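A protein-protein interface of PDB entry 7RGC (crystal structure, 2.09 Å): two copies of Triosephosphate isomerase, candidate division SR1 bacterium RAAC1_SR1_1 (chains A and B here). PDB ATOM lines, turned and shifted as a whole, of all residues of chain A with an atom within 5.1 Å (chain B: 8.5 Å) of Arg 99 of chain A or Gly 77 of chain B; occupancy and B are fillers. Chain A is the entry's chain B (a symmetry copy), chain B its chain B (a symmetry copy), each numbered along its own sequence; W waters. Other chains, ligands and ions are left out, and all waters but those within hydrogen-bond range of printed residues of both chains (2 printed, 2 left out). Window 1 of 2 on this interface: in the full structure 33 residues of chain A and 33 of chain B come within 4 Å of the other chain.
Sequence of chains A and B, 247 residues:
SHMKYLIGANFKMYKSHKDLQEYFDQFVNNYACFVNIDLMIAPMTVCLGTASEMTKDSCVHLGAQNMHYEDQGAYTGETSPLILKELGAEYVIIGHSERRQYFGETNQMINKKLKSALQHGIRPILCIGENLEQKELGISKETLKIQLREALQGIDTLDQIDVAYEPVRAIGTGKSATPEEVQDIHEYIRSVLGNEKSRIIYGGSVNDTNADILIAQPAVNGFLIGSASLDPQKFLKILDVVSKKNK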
ATOM      1  N   THR A  45     -22.286 -24.235   1.066  1.00  0.00           N
ATOM      2  CA  THR A  45     -21.149 -24.635   1.898  1.00  0.00           C
ATOM      3  C   THR A  45     -21.587 -25.104   3.286  1.00  0.00           C
ATOM      4  O   THR A  45     -21.004 -26.038   3.847  1.00  0.00           O
ATOM      5  CB  THR A  45     -20.173 -23.465   2.020  1.00  0.00           C
ATOM      6  OG1 THR A  45     -19.594 -23.205   0.744  1.00  0.00           O
ATOM      7  CG2 THR A  45     -19.064 -23.753   3.031  1.00  0.00           C
ATOM      8  N   GLN A  65     -18.355 -24.735  -3.311  1.00  0.00           N
ATOM      9  CA  GLN A  65     -18.578 -23.550  -4.136  1.00  0.00           C
ATOM     10  C   GLN A  65     -17.480 -22.499  -3.992  1.00  0.00           C
ATOM     11  O   GLN A  65     -17.391 -21.593  -4.831  1.00  0.00           O
ATOM     12  CB  GLN A  65     -19.945 -22.942  -3.805  1.00  0.00           C
ATOM     13  CG  GLN A  65     -21.109 -23.777  -4.327  1.00  0.00           C
ATOM     14  CD  GLN A  65     -22.457 -23.272  -3.866  1.00  0.00           C
ATOM     15  OE1 GLN A  65     -22.596 -22.121  -3.457  1.00  0.00           O
ATOM     16  NE2 GLN A  65     -23.464 -24.136  -3.931  1.00  0.00           N
ATOM     17  N   ASN A  66     -16.649 -22.596  -2.960  1.00  0.00           N
ATOM     18  CA  ASN A  66     -15.614 -21.607  -2.688  1.00  0.00           C
ATOM     19  C   ASN A  66     -14.709 -22.198  -1.624  1.00  0.00           C
ATOM     20  O   ASN A  66     -15.003 -23.244  -1.047  1.00  0.00           O
ATOM     21  CB  ASN A  66     -16.208 -20.272  -2.227  1.00  0.00           C
ATOM     22  CG  ASN A  66     -15.150 -19.167  -2.082  1.00  0.00           C
ATOM     23  OD1 ASN A  66     -14.157 -19.134  -2.810  1.00  0.00           O
ATOM     24  ND2 ASN A  66     -15.351 -18.283  -1.116  1.00  0.00           N
ATOM     25  N   GLU A  78     -14.689 -17.776   6.461  1.00  0.00           N
ATOM     26  CA  GLU A  78     -14.081 -18.508   5.360  1.00  0.00           C
ATOM     27  C   GLU A  78     -14.054 -20.004   5.650  1.00  0.00           C
ATOM     28  O   GLU A  78     -14.297 -20.456   6.776  1.00  0.00           O
ATOM     29  CB  GLU A  78     -12.670 -17.989   5.093  1.00  0.00           C
ATOM     30  CG  GLU A  78     -12.649 -16.592   4.508  1.00  0.00           C
ATOM     31  CD  GLU A  78     -13.398 -16.501   3.185  1.00  0.00           C
ATOM     32  OE1 GLU A  78     -12.868 -17.011   2.184  1.00  0.00           O
ATOM     33  OE2 GLU A  78     -14.510 -15.920   3.146  1.00  0.00           O
ATOM     34  N   GLY A  95     -13.292 -18.730  -8.228  1.00  0.00           N
ATOM     35  CA  GLY A  95     -13.439 -17.545  -9.045  1.00  0.00           C
ATOM     36  C   GLY A  95     -14.704 -17.470  -9.867  1.00  0.00           C
ATOM     37  O   GLY A  95     -14.701 -16.847 -10.937  1.00  0.00           O
ATOM     38  N   HIS A  96     -15.781 -18.098  -9.410  1.00  0.00           N
ATOM     39  CA  HIS A  96     -17.094 -17.880 -10.001  1.00  0.00           C
ATOM     40  C   HIS A  96     -17.397 -16.390 -10.133  1.00  0.00           C
ATOM     41  O   HIS A  96     -17.065 -15.593  -9.249  1.00  0.00           O
ATOM     42  CB  HIS A  96     -18.164 -18.549  -9.135  1.00  0.00           C
ATOM     43  CG  HIS A  96     -19.487 -18.676  -9.820  1.00  0.00           C
ATOM     44  ND1 HIS A  96     -20.414 -17.655  -9.843  1.00  0.00           N
ATOM     45  CD2 HIS A  96     -20.034 -19.700 -10.519  1.00  0.00           C
ATOM     46  CE1 HIS A  96     -21.474 -18.046 -10.532  1.00  0.00           C
ATOM     47  NE2 HIS A  96     -21.267 -19.280 -10.955  1.00  0.00           N
ATOM     48  N   SER A  97     -18.067 -16.023 -11.235  1.00  0.00           N
ATOM     49  CA  SER A  97     -18.369 -14.620 -11.505  1.00  0.00           C
ATOM     50  C   SER A  97     -19.117 -13.948 -10.357  1.00  0.00           C
ATOM     51  O   SER A  97     -18.942 -12.740 -10.123  1.00  0.00           O
ATOM     52  CB  SER A  97     -19.171 -14.490 -12.803  1.00  0.00           C
ATOM     53  OG  SER A  97     -20.544 -14.780 -12.619  1.00  0.00           O
ATOM     54  N   GLU A  98     -19.941 -14.700  -9.615  1.00  0.00           N
ATOM     55  CA  GLU A  98     -20.651 -14.058  -8.513  1.00  0.00           C
ATOM     56  C   GLU A  98     -19.697 -13.657  -7.391  1.00  0.00           C
ATOM     57  O   GLU A  98     -19.906 -12.616  -6.758  1.00  0.00           O
ATOM     58  CB  GLU A  98     -21.768 -14.966  -8.006  1.00  0.00           C
ATOM     59  CG  GLU A  98     -22.995 -14.979  -8.916  1.00  0.00           C
ATOM     60  CD  GLU A  98     -23.698 -16.325  -8.921  1.00  0.00           C
ATOM     61  OE1 GLU A  98     -23.499 -17.103  -7.959  1.00  0.00           O
ATOM     62  OE2 GLU A  98     -24.442 -16.614  -9.886  1.00  0.00           O
ATOM     63  N   ARG A  99     -18.634 -14.442  -7.148  1.00  0.00           N
ATOM     64  CA  ARG A  99     -17.621 -14.028  -6.177  1.00  0.00           C
ATOM     65  C   ARG A  99     -16.860 -12.802  -6.661  1.00  0.00           C
ATOM     66  O   ARG A  99     -16.478 -11.951  -5.851  1.00  0.00           O
ATOM     67  CB  ARG A  99     -16.608 -15.134  -5.894  1.00  0.00           C
ATOM     68  CG  ARG A  99     -17.150 -16.514  -5.653  1.00  0.00           C
ATOM     69  CD  ARG A  99     -17.855 -16.659  -4.354  1.00  0.00           C
ATOM     70  NE  ARG A  99     -17.170 -16.142  -3.167  1.00  0.00           N
ATOM     71  CZ  ARG A  99     -17.796 -15.931  -2.010  1.00  0.00           C
ATOM     72  NH1 ARG A  99     -19.095 -16.190  -1.919  1.00  0.00           N
ATOM     73  NH2 ARG A  99     -17.145 -15.465  -0.949  1.00  0.00           N
ATOM     74  N   ARG A 100     -16.574 -12.729  -7.967  1.00  0.00           N
ATOM     75  CA  ARG A 100     -15.875 -11.561  -8.495  1.00  0.00           C
ATOM     76  C   ARG A 100     -16.734 -10.307  -8.387  1.00  0.00           C
ATOM     77  O   ARG A 100     -16.224  -9.222  -8.081  1.00  0.00           O
ATOM     78  CB  ARG A 100     -15.470 -11.784  -9.955  1.00  0.00           C
ATOM     79  CG  ARG A 100     -14.564 -12.986 -10.228  1.00  0.00           C
ATOM     80  CD  ARG A 100     -14.521 -13.266 -11.739  1.00  0.00           C
ATOM     81  NE  ARG A 100     -13.758 -14.466 -12.114  1.00  0.00           N
ATOM     82  CZ  ARG A 100     -12.458 -14.447 -12.403  1.00  0.00           C
ATOM     83  NH1 ARG A 100     -11.779 -13.299 -12.350  1.00  0.00           N
ATOM     84  NH2 ARG A 100     -11.834 -15.558 -12.745  1.00  0.00           N
ATOM     85  N   GLN A 101     -18.037 -10.432  -8.653  1.00  0.00           N
ATOM     86  CA  GLN A 101     -18.887  -9.248  -8.690  1.00  0.00           C
ATOM     87  C   GLN A 101     -19.224  -8.753  -7.289  1.00  0.00           C
ATOM     88  O   GLN A 101     -19.202  -7.544  -7.042  1.00  0.00           O
ATOM     89  CB  GLN A 101     -20.173  -9.537  -9.467  1.00  0.00           C
ATOM     90  CG  GLN A 101     -21.276  -8.498  -9.235  1.00  0.00           C
ATOM     91  CD  GLN A 101     -22.674  -9.018  -9.555  1.00  0.00           C
ATOM     92  OE1 GLN A 101     -22.879 -10.213  -9.717  1.00  0.00           O
ATOM     93  NE2 GLN A 101     -23.643  -8.114  -9.623  1.00  0.00           N
ATOM     94  N   TYR A 102     -19.513  -9.663  -6.354  1.00  0.00           N
ATOM     95  CA  TYR A 102     -20.110  -9.291  -5.073  1.00  0.00           C
ATOM     96  C   TYR A 102     -19.149  -9.296  -3.897  1.00  0.00           C
ATOM     97  O   TYR A 102     -19.387  -8.568  -2.930  1.00  0.00           O
ATOM     98  CB  TYR A 102     -21.255 -10.239  -4.717  1.00  0.00           C
ATOM     99  CG  TYR A 102     -22.541 -10.042  -5.478  1.00  0.00           C
ATOM    100  CD1 TYR A 102     -23.203  -8.828  -5.453  1.00  0.00           C
ATOM    101  CD2 TYR A 102     -23.118 -11.097  -6.196  1.00  0.00           C
ATOM    102  CE1 TYR A 102     -24.391  -8.647  -6.136  1.00  0.00           C
ATOM    103  CE2 TYR A 102     -24.310 -10.928  -6.883  1.00  0.00           C
ATOM    104  CZ  TYR A 102     -24.940  -9.692  -6.848  1.00  0.00           C
ATOM    105  OH  TYR A 102     -26.128  -9.490  -7.516  1.00  0.00           O
ATOM    106  N   PHE A 103     -18.102 -10.123  -3.905  1.00  0.00           N
ATOM    107  CA  PHE A 103     -17.412 -10.392  -2.645  1.00  0.00           C
ATOM    108  C   PHE A 103     -15.894 -10.251  -2.746  1.00  0.00           C
ATOM    109  O   PHE A 103     -15.155 -10.986  -2.081  1.00  0.00           O
ATOM    110  CB  PHE A 103     -17.786 -11.778  -2.122  1.00  0.00           C
ATOM    111  CG  PHE A 103     -19.268 -12.017  -2.069  1.00  0.00           C
ATOM    112  CD1 PHE A 103     -20.068 -11.320  -1.162  1.00  0.00           C
ATOM    113  CD2 PHE A 103     -19.865 -12.921  -2.921  1.00  0.00           C
ATOM    114  CE1 PHE A 103     -21.435 -11.530  -1.112  1.00  0.00           C
ATOM    115  CE2 PHE A 103     -21.227 -13.129  -2.880  1.00  0.00           C
ATOM    116  CZ  PHE A 103     -22.015 -12.439  -1.974  1.00  0.00           C
ATOM    117  N   GLY A 104     -15.413  -9.307  -3.551  1.00  0.00           N
ATOM    118  CA  GLY A 104     -13.990  -9.016  -3.560  1.00  0.00           C
ATOM    119  C   GLY A 104     -13.072 -10.113  -4.062  1.00  0.00           C
ATOM    120  O   GLY A 104     -11.875 -10.100  -3.742  1.00  0.00           O
ATOM    121  N   GLU A 105     -13.584 -11.067  -4.840  1.00  0.00           N
ATOM    122  CA  GLU A 105     -12.723 -12.082  -5.437  1.00  0.00           C
ATOM    123  C   GLU A 105     -11.870 -11.466  -6.548  1.00  0.00           C
ATOM    124  O   GLU A 105     -12.403 -10.964  -7.544  1.00  0.00           O
ATOM    125  CB  GLU A 105     -13.568 -13.228  -5.988  1.00  0.00           C
ATOM    126  CG  GLU A 105     -12.807 -14.503  -6.260  1.00  0.00           C
ATOM    127  CD  GLU A 105     -12.758 -15.431  -5.055  1.00  0.00           C
ATOM    128  OE1 GLU A 105     -13.764 -15.545  -4.311  1.00  0.00           O
ATOM    129  OE2 GLU A 105     -11.705 -16.066  -4.855  1.00  0.00           O
ATOM    130  N   THR B  45     -17.906 -21.988   9.209  1.00  0.00           N
ATOM    131  CA  THR B  45     -19.246 -22.184   8.650  1.00  0.00           C
ATOM    132  C   THR B  45     -19.450 -23.607   8.131  1.00  0.00           C
ATOM    133  O   THR B  45     -20.544 -24.172   8.257  1.00  0.00           O
ATOM    134  CB  THR B  45     -19.480 -21.173   7.528  1.00  0.00           C
ATOM    135  OG1 THR B  45     -19.526 -19.861   8.082  1.00  0.00           O
ATOM    136  CG2 THR B  45     -20.782 -21.451   6.776  1.00  0.00           C
ATOM    137  N   ASN B  66     -20.774 -15.479   9.497  1.00  0.00           N
ATOM    138  CA  ASN B  66     -21.185 -14.634   8.383  1.00  0.00           C
ATOM    139  C   ASN B  66     -22.485 -15.207   7.852  1.00  0.00           C
ATOM    140  O   ASN B  66     -22.915 -16.288   8.252  1.00  0.00           O
ATOM    141  CB  ASN B  66     -20.119 -14.579   7.285  1.00  0.00           C
ATOM    142  CG  ASN B  66     -20.460 -13.576   6.172  1.00  0.00           C
ATOM    143  OD1 ASN B  66     -21.093 -12.546   6.412  1.00  0.00           O
ATOM    144  ND2 ASN B  66     -20.068 -13.897   4.948  1.00  0.00           N
ATOM    145  N   MET B  67     -23.083 -14.495   6.911  1.00  0.00           N
ATOM    146  CA  MET B  67     -24.424 -14.818   6.457  1.00  0.00           C
ATOM    147  C   MET B  67     -24.741 -13.908   5.288  1.00  0.00           C
ATOM    148  O   MET B  67     -24.320 -12.755   5.288  1.00  0.00           O
ATOM    149  CB  MET B  67     -25.412 -14.588   7.592  1.00  0.00           C
ATOM    150  CG  MET B  67     -26.854 -14.660   7.239  1.00  0.00           C
ATOM    151  SD  MET B  67     -27.815 -14.211   8.707  1.00  0.00           S
ATOM    152  CE  MET B  67     -28.590 -12.754   8.008  1.00  0.00           C
ATOM    153  N   HIS B  68     -25.455 -14.425   4.291  1.00  0.00           N
ATOM    154  CA  HIS B  68     -25.936 -13.552   3.229  1.00  0.00           C
ATOM    155  C   HIS B  68     -27.213 -12.852   3.680  1.00  0.00           C
ATOM    156  O   HIS B  68     -27.801 -13.185   4.710  1.00  0.00           O
ATOM    157  CB  HIS B  68     -26.192 -14.339   1.942  1.00  0.00           C
ATOM    158  CG  HIS B  68     -26.224 -13.479   0.714  1.00  0.00           C
ATOM    159  ND1 HIS B  68     -27.395 -13.155   0.064  1.00  0.00           N
ATOM    160  CD2 HIS B  68     -25.234 -12.842   0.047  1.00  0.00           C
ATOM    161  CE1 HIS B  68     -27.122 -12.368  -0.962  1.00  0.00           C
ATOM    162  NE2 HIS B  68     -25.817 -12.165  -0.997  1.00  0.00           N
ATOM    163  N   GLY B  73     -30.666 -17.750  -3.574  1.00  0.00           N
ATOM    164  CA  GLY B  73     -30.447 -17.163  -4.878  1.00  0.00           C
ATOM    165  C   GLY B  73     -29.044 -17.434  -5.379  1.00  0.00           C
ATOM    166  O   GLY B  73     -28.314 -18.260  -4.830  1.00  0.00           O
ATOM    167  N   ALA B  74     -28.691 -16.707  -6.443  1.00  0.00           N
ATOM    168  CA  ALA B  74     -27.473 -16.957  -7.212  1.00  0.00           C
ATOM    169  C   ALA B  74     -26.284 -16.271  -6.541  1.00  0.00           C
ATOM    170  O   ALA B  74     -25.748 -15.266  -7.015  1.00  0.00           O
ATOM    171  CB  ALA B  74     -27.653 -16.474  -8.644  1.00  0.00           C
ATOM    172  N   TYR B  75     -25.877 -16.828  -5.401  1.00  0.00           N
ATOM    173  CA  TYR B  75     -24.813 -16.249  -4.584  1.00  0.00           C
ATOM    174  C   TYR B  75     -23.817 -17.357  -4.260  1.00  0.00           C
ATOM    175  O   TYR B  75     -23.741 -17.840  -3.127  1.00  0.00           O
ATOM    176  CB  TYR B  75     -25.375 -15.587  -3.325  1.00  0.00           C
ATOM    177  CG  TYR B  75     -26.450 -14.582  -3.656  1.00  0.00           C
ATOM    178  CD1 TYR B  75     -26.114 -13.324  -4.174  1.00  0.00           C
ATOM    179  CD2 TYR B  75     -27.799 -14.883  -3.464  1.00  0.00           C
ATOM    180  CE1 TYR B  75     -27.090 -12.396  -4.496  1.00  0.00           C
ATOM    181  CE2 TYR B  75     -28.788 -13.957  -3.789  1.00  0.00           C
ATOM    182  CZ  TYR B  75     -28.424 -12.718  -4.313  1.00  0.00           C
ATOM    183  OH  TYR B  75     -29.391 -11.798  -4.645  1.00  0.00           O
ATOM    184  N   THR B  76     -23.047 -17.742  -5.273  1.00  0.00           N
ATOM    185  CA  THR B  76     -22.132 -18.867  -5.141  1.00  0.00           C
ATOM    186  C   THR B  76     -21.216 -18.681  -3.941  1.00  0.00           C
ATOM    187  O   THR B  76     -20.569 -17.641  -3.797  1.00  0.00           O
ATOM    188  CB  THR B  76     -21.310 -19.026  -6.429  1.00  0.00           C
ATOM    189  OG1 THR B  76     -22.168 -19.498  -7.471  1.00  0.00           O
ATOM    190  CG2 THR B  76     -20.140 -19.994  -6.237  1.00  0.00           C
ATOM    191  N   GLY B  77     -21.199 -19.690  -3.062  1.00  0.00           N
ATOM    192  CA  GLY B  77     -20.338 -19.703  -1.895  1.00  0.00           C
ATOM    193  C   GLY B  77     -20.904 -19.036  -0.666  1.00  0.00           C
ATOM    194  O   GLY B  77     -20.210 -18.976   0.362  1.00  0.00           O
ATOM    195  N   GLU B  78     -22.137 -18.543  -0.730  1.00  0.00           N
ATOM    196  CA  GLU B  78     -22.755 -17.843   0.384  1.00  0.00           C
ATOM    197  C   GLU B  78     -23.613 -18.790   1.216  1.00  0.00           C
ATOM    198  O   GLU B  78     -23.908 -19.923   0.818  1.00  0.00           O
ATOM    199  CB  GLU B  78     -23.591 -16.670  -0.123  1.00  0.00           C
ATOM    200  CG  GLU B  78     -22.755 -15.545  -0.695  1.00  0.00           C
ATOM    201  CD  GLU B  78     -21.779 -14.967   0.320  1.00  0.00           C
ATOM    202  OE1 GLU B  78     -22.244 -14.262   1.231  1.00  0.00           O
ATOM    203  OE2 GLU B  78     -20.555 -15.214   0.206  1.00  0.00           O
ATOM    204  N   THR B  79     -24.025 -18.293   2.387  1.00  0.00           N
ATOM    205  CA  THR B  79     -24.703 -19.083   3.414  1.00  0.00           C
ATOM    206  C   THR B  79     -26.074 -18.479   3.683  1.00  0.00           C
ATOM    207  O   THR B  79     -26.183 -17.281   3.971  1.00  0.00           O
ATOM    208  CB  THR B  79     -23.878 -19.132   4.712  1.00  0.00           C
ATOM    209  OG1 THR B  79     -22.688 -19.895   4.492  1.00  0.00           O
ATOM    210  CG2 THR B  79     -24.665 -19.782   5.825  1.00  0.00           C
ATOM    211  N   SER B  80     -27.113 -19.303   3.595  1.00  0.00           N
ATOM    212  CA  SER B  80     -28.429 -18.681   3.685  1.00  0.00           C
ATOM    213  C   SER B  80     -28.909 -18.632   5.134  1.00  0.00           C
ATOM    214  O   SER B  80     -28.701 -19.588   5.890  1.00  0.00           O
ATOM    215  CB  SER B  80     -29.441 -19.447   2.842  1.00  0.00           C
ATOM    216  OG  SER B  80     -30.768 -19.144   3.234  1.00  0.00           O
ATOM    217  N   ARG B  99     -13.970  -9.454   7.179  1.00  0.00           N
ATOM    218  CA  ARG B  99     -14.822  -9.396   5.992  1.00  0.00           C
ATOM    219  C   ARG B  99     -14.708  -8.048   5.295  1.00  0.00           C
ATOM    220  O   ARG B  99     -14.778  -7.980   4.063  1.00  0.00           O
ATOM    221  CB  ARG B  99     -16.293  -9.635   6.325  1.00  0.00           C
ATOM    222  CG  ARG B  99     -16.609 -10.781   7.244  1.00  0.00           C
ATOM    223  CD  ARG B  99     -16.407 -12.115   6.623  1.00  0.00           C
ATOM    224  NE  ARG B  99     -16.987 -12.322   5.294  1.00  0.00           N
ATOM    225  CZ  ARG B  99     -16.633 -13.337   4.506  1.00  0.00           C
ATOM    226  NH1 ARG B  99     -15.715 -14.197   4.929  1.00  0.00           N
ATOM    227  NH2 ARG B  99     -17.181 -13.500   3.307  1.00  0.00           N
ATOM    228  N   TYR B 102     -10.982  -8.025   3.536  1.00  0.00           N
ATOM    229  CA  TYR B 102     -10.598  -9.028   2.546  1.00  0.00           C
ATOM    230  C   TYR B 102     -11.672  -9.352   1.521  1.00  0.00           C
ATOM    231  O   TYR B 102     -11.330  -9.773   0.413  1.00  0.00           O
ATOM    232  CB  TYR B 102     -10.223 -10.343   3.228  1.00  0.00           C
ATOM    233  CG  TYR B 102      -8.880 -10.376   3.914  1.00  0.00           C
ATOM    234  CD1 TYR B 102      -7.717 -10.116   3.211  1.00  0.00           C
ATOM    235  CD2 TYR B 102      -8.777 -10.711   5.269  1.00  0.00           C
ATOM    236  CE1 TYR B 102      -6.484 -10.160   3.832  1.00  0.00           C
ATOM    237  CE2 TYR B 102      -7.544 -10.760   5.901  1.00  0.00           C
ATOM    238  CZ  TYR B 102      -6.398 -10.480   5.171  1.00  0.00           C
ATOM    239  OH  TYR B 102      -5.156 -10.524   5.766  1.00  0.00           O
ATOM    240  N   PHE B 103     -12.958  -9.230   1.852  1.00  0.00           N
ATOM    241  CA  PHE B 103     -13.962  -9.885   1.016  1.00  0.00           C
ATOM    242  C   PHE B 103     -15.119  -8.965   0.631  1.00  0.00           C
ATOM    243  O   PHE B 103     -16.264  -9.420   0.511  1.00  0.00           O
ATOM    244  CB  PHE B 103     -14.487 -11.143   1.706  1.00  0.00           C
ATOM    245  CG  PHE B 103     -13.398 -12.061   2.184  1.00  0.00           C
ATOM    246  CD1 PHE B 103     -12.594 -12.744   1.270  1.00  0.00           C
ATOM    247  CD2 PHE B 103     -13.168 -12.237   3.531  1.00  0.00           C
ATOM    248  CE1 PHE B 103     -11.584 -13.586   1.703  1.00  0.00           C
ATOM    249  CE2 PHE B 103     -12.160 -13.069   3.968  1.00  0.00           C
ATOM    250  CZ  PHE B 103     -11.368 -13.749   3.057  1.00  0.00           C
ATOM    251  N   GLY B 104     -14.844  -7.682   0.412  1.00  0.00           N
ATOM    252  CA  GLY B 104     -15.867  -6.798  -0.117  1.00  0.00           C
ATOM    253  C   GLY B 104     -17.069  -6.538   0.770  1.00  0.00           C
ATOM    254  O   GLY B 104     -18.126  -6.140   0.260  1.00  0.00           O
HETATM  255  O   HOH W   1     -22.602 -21.841  -0.425  1.00  0.00           O
HETATM  256  O   HOH W   2     -16.067 -19.902   8.644  1.00  0.00           O
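The backbone carbonyl oxygen (O) of Phe 103 of chain A sits close to the backbone carbonyl oxygen (O) of Phe 103 of chain B (3.2 Å). OE2 of Glu 78 of chain B lies within salt-bridge range of NH1 of Arg 99 of chain A (2.8 Å). OG1 of Thr 76 of chain B lies within hydrogen-bond range of OE1 of Glu 98 of chain A (2.8 Å). The side-chain carboxylate (OE1) of Glu 98 of chain A lies close to the backbone carbonyl oxygen (O) of Ala 74 of chain B. The side-chain amide oxygen (OE1) of Gln 65 of chain A is in hydrogen-bond range of the backbone NH (N) of Gly 77 of chain B, at 2.8 Å. NH1 of Arg 99 of chain A lies within hydrogen-bond range of O of Thr 76 of chain B (2.8 Å). The guanidinium group (NH1) of Arg 99 of chain B is in salt-bridge range of the side-chain carboxylate (OE2) of Glu 78 of chain A (2.8 Å). A ring nitrogen (ND1) of His 96 of chain A sits close to the side-chain hydroxyl of Thr 76 of chain B, at 3.5 Å.
The guanidinium group (NH2) of Arg 99 of chain A sits close to the side-chain amide nitrogen (ND2) of Asn 66 of chain A, at 3.3 Å. ND2 of Asn 66 of chain B lies close to NH2 of Arg 99 of chain B (3.3 Å). The backbone NH of Glu 98 of chain A is in hydrogen-bond range of a ring nitrogen (ND1) of His 96 of chain A, 3.0 Å away. OE1 of Glu 105 of chain A is in salt-bridge range of NE of Arg 99 of chain A, 3.6 Å away. The backbone carbonyl oxygen of Thr 79 of chain B is in hydrogen-bond range of the backbone NH of His 68 of chain B, 3.0 Å away.
Among the printed residues, pairs that only touch across the chains: Phe 103 of chain A with Glu 78 of chain B, Glu 78 of chain A with Phe 103 of chain B, Gln 65 of chain A with Thr 76 of chain B, Glu 98 of chain A with Tyr 75 of chain B, Arg 99 of chain A with Gly 77 of chain B, Phe 103 of chain A with His 68 of chain B and Tyr 102 of chain A with Tyr 75 of chain B.
Ser 97 of chain A touches none of the printed residues of chain B. Printed residues of chain B within 4 Å of Arg 99 of chain A: Thr 76, Gly 77 and Glu 78. Printed residues of chain B within 4 Å of Tyr 102 of chain A: Tyr 75. Printed residues of chain B within 4 Å of Phe 103 of chain A: His 68, Glu 78 and Phe 103. Thr 45 of chain B touches none of the printed residues of chain A. Gly 77 of chain B touches just these residues of chain A: Gln 65 (2.8 Å) and Arg 99 (3.6 Å). Of the printed residues of chain A, Glu 78 of chain B touches Arg 99 (2.8 Å) and Phe 103 (3.4 Å). Printed residues of chain A within 4 Å of Arg 99 of chain B: Glu 78. The nearest residue of chain B that does not touch Arg 99 of chain A is Arg 99 of chain B (4.7 Å). The nearest residue of chain A that does not touch Gly 77 of chain B is Asn 66 of chain A (4.2 Å). The nearest printed residue of chain B that does not touch Tyr 102 of chain A is Gly 104 of chain B (4.2 Å).
Hydrophobic or aromatic side chains of chain A that line the printed part of chain B: His 96, Tyr 102 and Phe 103. Of the 16 printed residues of chain B, 8 touch a printed residue of chain A. Printed residues of chain B that touch a printed residue of chain A: His 68, Ala 74, Tyr 75, Thr 76, Gly 77, Glu 78, Arg 99 and Phe 103. Among the printed residues, 15 pairs touch across the chains. Among the printed residues, Asp or Glu carboxylates within 4 Å of a Lys or Arg side-chain nitrogen of the other chain: Glu 78 of chain A with Arg 99 of chain B and Arg 99 of chain A with Glu 78 of chain B.
Glu 78 of chain A touches Arg 99 of chain B, and with the chains exchanged Arg 99 of chain A touches Glu 78 of chain B. Glu 78 of chain A touches Phe 103 of chain B, and with the chains exchanged Phe 103 of chain A touches Glu 78 of chain B. Phe 103 of chain B touches its own counterpart, Phe 103 of chain A. Of the 15 pairs that touch across the chains among the printed residues, 5 have their exchanged pair printed and touching as well.
Water W2 lies within hydrogen-bond range of O of Glu 78 of chain A (2.6 Å) and N of Thr 45 of chain B (2.8 Å). Water W1 lies within hydrogen-bond range of the backbone carbonyl oxygen (O) of Glu 78 of chain B (2.6 Å), the backbone NH (N) of Thr 45 of chain A (2.8 Å) and the side-chain amide oxygen (OE1) of Gln 65 of chain A (3.0 Å).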
